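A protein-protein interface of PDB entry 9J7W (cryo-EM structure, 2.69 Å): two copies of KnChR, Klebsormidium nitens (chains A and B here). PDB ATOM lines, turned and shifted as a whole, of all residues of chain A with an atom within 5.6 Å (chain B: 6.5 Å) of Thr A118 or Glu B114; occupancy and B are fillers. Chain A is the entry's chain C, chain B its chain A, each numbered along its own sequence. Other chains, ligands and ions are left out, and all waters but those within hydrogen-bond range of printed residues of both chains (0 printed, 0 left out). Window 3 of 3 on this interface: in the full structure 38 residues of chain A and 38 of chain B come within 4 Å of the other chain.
The backbone NH of Gly B112 lies close to the side-chain amide oxygen of Asn B109 (3.1 Å). The side-chain hydroxyl of Tyr B117 sits close to the side-chain amide nitrogen of Asn B109 (3.4 Å). OG1 of Thr A118 lies close to N of Arg A120 (3.5 Å).
Among the printed residues, pairs that only touch across the chains: Tyr A117 with Tyr B117, Tyr A117 with Met B122, Thr A118 with Glu B114, His A119 with Gly B112, His A119 with Glu B113, His A119 with Tyr B117, Met A122 with Tyr B117 and Met A122 with Met B122.
Thr A118 touches just one residue of chain B: Glu B114. Of chain A, only Thr A118 and His A119 come within 4 Å of Glu B114. Of the printed residues of chain B, Tyr A117 touches Tyr B117 and Met B122. Of the printed residues of chain A, Glu B113 touches His A119. Printed residues of chain A within 4 Å of Tyr B117: Tyr A117, His A119 and Met A122. Ser A121 touches none of the printed residues of chain B.
NE2 of His A119 lies within hydrogen-bond range of ND2 of Asn B109, at 2.9 Å. A ring nitrogen (ND1) of His A119 is in hydrogen-bond range of the side-chain carboxylate of Glu B114 (3.3 Å).
Tyr B117 touches its own counterpart, Tyr A117. Tyr A117 touches Met B122, and with the chains exchanged Met A122 touches Tyr B117. Met A122 touches its own counterpart, Met B122.
Printed residues of chain B that touch a printed residue of chain A: Asn B109, Gly B112, Glu B113, Glu B114, Tyr B117 and Met B122. Hydrophobic or aromatic side chains of chain B that line the printed part of chain A: Tyr B117 and Met B122. Among the printed residues, no Asp or Glu carboxylate lies within 4 Å of a Lys or Arg side-chain nitrogen of the other chain.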
ATOM      1  N   GLU A 116      11.787  21.053 -16.057  1.00  0.00           N
ATOM      2  CA  GLU A 116      10.902  21.012 -14.902  1.00  0.00           C
ATOM      3  C   GLU A 116      10.410  19.611 -14.574  1.00  0.00           C
ATOM      4  O   GLU A 116       9.900  19.396 -13.470  1.00  0.00           O
ATOM      5  CB  GLU A 116       9.692  21.925 -15.130  1.00  0.00           C
ATOM      6  CG  GLU A 116       9.940  23.385 -14.783  1.00  0.00           C
ATOM      7  CD  GLU A 116       8.664  24.134 -14.446  1.00  0.00           C
ATOM      8  OE1 GLU A 116       7.569  23.554 -14.604  1.00  0.00           O
ATOM      9  OE2 GLU A 116       8.756  25.306 -14.021  1.00  0.00           O
ATOM     10  N   TYR A 117      10.546  18.664 -15.495  1.00  0.00           N
ATOM     11  CA  TYR A 117      10.160  17.291 -15.219  1.00  0.00           C
ATOM     12  C   TYR A 117      11.120  16.651 -14.222  1.00  0.00           C
ATOM     13  O   TYR A 117      12.270  17.066 -14.064  1.00  0.00           O
ATOM     14  CB  TYR A 117      10.124  16.469 -16.505  1.00  0.00           C
ATOM     15  CG  TYR A 117       9.013  16.835 -17.456  1.00  0.00           C
ATOM     16  CD1 TYR A 117       7.686  16.648 -17.101  1.00  0.00           C
ATOM     17  CD2 TYR A 117       9.285  17.347 -18.715  1.00  0.00           C
ATOM     18  CE1 TYR A 117       6.666  16.969 -17.966  1.00  0.00           C
ATOM     19  CE2 TYR A 117       8.268  17.669 -19.588  1.00  0.00           C
ATOM     20  CZ  TYR A 117       6.961  17.476 -19.206  1.00  0.00           C
ATOM     21  OH  TYR A 117       5.942  17.794 -20.069  1.00  0.00           O
ATOM     22  N   THR A 118      10.626  15.619 -13.542  1.00  0.00           N
ATOM     23  CA  THR A 118      11.382  14.946 -12.498  1.00  0.00           C
ATOM     24  C   THR A 118      11.067  13.458 -12.533  1.00  0.00           C
ATOM     25  O   THR A 118      10.190  13.001 -13.270  1.00  0.00           O
ATOM     26  CB  THR A 118      11.067  15.524 -11.114  1.00  0.00           C
ATOM     27  OG1 THR A 118       9.695  15.269 -10.790  1.00  0.00           O
ATOM     28  CG2 THR A 118      11.322  17.017 -11.084  1.00  0.00           C
ATOM     29  N   HIS A 119      11.805  12.701 -11.719  1.00  0.00           N
ATOM     30  CA  HIS A 119      11.563  11.267 -11.615  1.00  0.00           C
ATOM     31  C   HIS A 119      10.182  10.993 -11.036  1.00  0.00           C
ATOM     32  O   HIS A 119       9.517  10.016 -11.408  1.00  0.00           O
ATOM     33  CB  HIS A 119      12.641  10.628 -10.743  1.00  0.00           C
ATOM     34  CG  HIS A 119      13.993  10.594 -11.381  1.00  0.00           C
ATOM     35  ND1 HIS A 119      15.089  11.218 -10.828  1.00  0.00           N
ATOM     36  CD2 HIS A 119      14.424  10.029 -12.532  1.00  0.00           C
ATOM     37  CE1 HIS A 119      16.140  11.030 -11.606  1.00  0.00           C
ATOM     38  NE2 HIS A 119      15.762  10.313 -12.647  1.00  0.00           N
ATOM     39  N   ARG A 120       9.741  11.846 -10.112  1.00  0.00           N
ATOM     40  CA  ARG A 120       8.439  11.686  -9.487  1.00  0.00           C
ATOM     41  C   ARG A 120       7.309  11.787 -10.499  1.00  0.00           C
ATOM     42  O   ARG A 120       6.274  11.145 -10.315  1.00  0.00           O
ATOM     43  CB  ARG A 120       8.279  12.734  -8.387  1.00  0.00           C
ATOM     44  CG  ARG A 120       9.288  12.573  -7.253  1.00  0.00           C
ATOM     45  CD  ARG A 120       9.045  11.305  -6.450  1.00  0.00           C
ATOM     46  NE  ARG A 120       7.725  11.322  -5.834  1.00  0.00           N
ATOM     47  CZ  ARG A 120       7.457  11.878  -4.660  1.00  0.00           C
ATOM     48  NH1 ARG A 120       8.412  12.388  -3.900  1.00  0.00           N
ATOM     49  NH2 ARG A 120       6.200  11.920  -4.236  1.00  0.00           N
ATOM     50  N   SER A 121       7.489  12.564 -11.568  1.00  0.00           N
ATOM     51  CA  SER A 121       6.500  12.591 -12.641  1.00  0.00           C
ATOM     52  C   SER A 121       6.344  11.215 -13.276  1.00  0.00           C
ATOM     53  O   SER A 121       5.223  10.751 -13.524  1.00  0.00           O
ATOM     54  CB  SER A 121       6.918  13.616 -13.692  1.00  0.00           C
ATOM     55  OG  SER A 121       6.924  14.925 -13.152  1.00  0.00           O
ATOM     56  N   MET A 122       7.463  10.549 -13.544  1.00  0.00           N
ATOM     57  CA  MET A 122       7.438   9.211 -14.115  1.00  0.00           C
ATOM     58  C   MET A 122       6.822   8.199 -13.159  1.00  0.00           C
ATOM     59  O   MET A 122       6.049   7.329 -13.581  1.00  0.00           O
ATOM     60  CB  MET A 122       8.860   8.814 -14.505  1.00  0.00           C
ATOM     61  CG  MET A 122       9.459   9.732 -15.547  1.00  0.00           C
ATOM     62  SD  MET A 122       8.641   9.567 -17.141  1.00  0.00           S
ATOM     63  CE  MET A 122       9.424  10.875 -18.062  1.00  0.00           C
ATOM     64  N   ASN B 109      16.039   7.711 -19.057  1.00  0.00           N
ATOM     65  CA  ASN B 109      16.836   7.958 -17.860  1.00  0.00           C
ATOM     66  C   ASN B 109      17.991   6.973 -17.778  1.00  0.00           C
ATOM     67  O   ASN B 109      18.266   6.378 -16.735  1.00  0.00           O
ATOM     68  CB  ASN B 109      15.984   7.860 -16.602  1.00  0.00           C
ATOM     69  CG  ASN B 109      16.673   8.437 -15.390  1.00  0.00           C
ATOM     70  OD1 ASN B 109      17.574   9.266 -15.509  1.00  0.00           O
ATOM     71  ND2 ASN B 109      16.277   7.973 -14.213  1.00  0.00           N
ATOM     72  N   GLY B 112      20.536   8.532 -15.146  1.00  0.00           N
ATOM     73  CA  GLY B 112      19.992   8.712 -13.816  1.00  0.00           C
ATOM     74  C   GLY B 112      20.025  10.131 -13.295  1.00  0.00           C
ATOM     75  O   GLY B 112      19.558  10.365 -12.173  1.00  0.00           O
ATOM     76  N   GLU B 113      20.550  11.087 -14.056  1.00  0.00           N
ATOM     77  CA  GLU B 113      20.623  12.451 -13.564  1.00  0.00           C
ATOM     78  C   GLU B 113      19.266  13.139 -13.676  1.00  0.00           C
ATOM     79  O   GLU B 113      18.326  12.643 -14.304  1.00  0.00           O
ATOM     80  CB  GLU B 113      21.672  13.258 -14.329  1.00  0.00           C
ATOM     81  CG  GLU B 113      23.101  12.804 -14.101  1.00  0.00           C
ATOM     82  CD  GLU B 113      23.479  11.629 -14.969  1.00  0.00           C
ATOM     83  OE1 GLU B 113      22.639  11.217 -15.790  1.00  0.00           O
ATOM     84  OE2 GLU B 113      24.610  11.118 -14.833  1.00  0.00           O
ATOM     85  N   GLU B 114      19.180  14.308 -13.052  1.00  0.00           N
ATOM     86  CA  GLU B 114      17.980  15.127 -13.054  1.00  0.00           C
ATOM     87  C   GLU B 114      18.091  16.180 -14.147  1.00  0.00           C
ATOM     88  O   GLU B 114      19.190  16.636 -14.475  1.00  0.00           O
ATOM     89  CB  GLU B 114      17.779  15.797 -11.693  1.00  0.00           C
ATOM     90  CG  GLU B 114      16.881  15.017 -10.752  1.00  0.00           C
ATOM     91  CD  GLU B 114      15.408  15.212 -11.052  1.00  0.00           C
ATOM     92  OE1 GLU B 114      14.839  16.228 -10.602  1.00  0.00           O
ATOM     93  OE2 GLU B 114      14.820  14.349 -11.735  1.00  0.00           O
ATOM     94  N   GLY B 115      16.950  16.559 -14.710  1.00  0.00           N
ATOM     95  CA  GLY B 115      16.921  17.541 -15.772  1.00  0.00           C
ATOM     96  C   GLY B 115      17.169  16.993 -17.158  1.00  0.00           C
ATOM     97  O   GLY B 115      17.192  17.771 -18.118  1.00  0.00           O
ATOM     98  N   GLU B 116      17.355  15.681 -17.297  1.00  0.00           N
ATOM     99  CA  GLU B 116      17.580  15.073 -18.600  1.00  0.00           C
ATOM    100  C   GLU B 116      16.293  14.721 -19.328  1.00  0.00           C
ATOM    101  O   GLU B 116      16.332  14.475 -20.538  1.00  0.00           O
ATOM    102  CB  GLU B 116      18.431  13.806 -18.453  1.00  0.00           C
ATOM    103  CG  GLU B 116      19.930  14.066 -18.408  1.00  0.00           C
ATOM    104  CD  GLU B 116      20.747  12.866 -18.848  1.00  0.00           C
ATOM    105  OE1 GLU B 116      20.157  11.786 -19.068  1.00  0.00           O
ATOM    106  OE2 GLU B 116      21.982  13.001 -18.974  1.00  0.00           O
ATOM    107  N   TYR B 117      15.162  14.691 -18.630  1.00  0.00           N
ATOM    108  CA  TYR B 117      13.890  14.430 -19.279  1.00  0.00           C
ATOM    109  C   TYR B 117      13.477  15.610 -20.153  1.00  0.00           C
ATOM    110  O   TYR B 117      13.907  16.749 -19.956  1.00  0.00           O
ATOM    111  CB  TYR B 117      12.803  14.146 -18.245  1.00  0.00           C
ATOM    112  CG  TYR B 117      12.959  12.839 -17.509  1.00  0.00           C
ATOM    113  CD1 TYR B 117      12.868  11.632 -18.183  1.00  0.00           C
ATOM    114  CD2 TYR B 117      13.174  12.808 -16.140  1.00  0.00           C
ATOM    115  CE1 TYR B 117      12.998  10.435 -17.518  1.00  0.00           C
ATOM    116  CE2 TYR B 117      13.305  11.612 -15.467  1.00  0.00           C
ATOM    117  CZ  TYR B 117      13.215  10.429 -16.162  1.00  0.00           C
ATOM    118  OH  TYR B 117      13.341   9.234 -15.501  1.00  0.00           O
ATOM    119  N   MET B 122       7.716  12.439 -22.947  1.00  0.00           N
ATOM    120  CA  MET B 122       6.285  12.343 -22.703  1.00  0.00           C
ATOM    121  C   MET B 122       5.517  11.994 -23.970  1.00  0.00           C
ATOM    122  O   MET B 122       4.582  11.182 -23.933  1.00  0.00           O
ATOM    123  CB  MET B 122       5.798  13.658 -22.104  1.00  0.00           C
ATOM    124  CG  MET B 122       6.455  13.978 -20.778  1.00  0.00           C
ATOM    125  SD  MET B 122       5.947  12.839 -19.483  1.00  0.00           S
ATOM    126  CE  MET B 122       7.010  13.347 -18.148  1.00  0.00           C
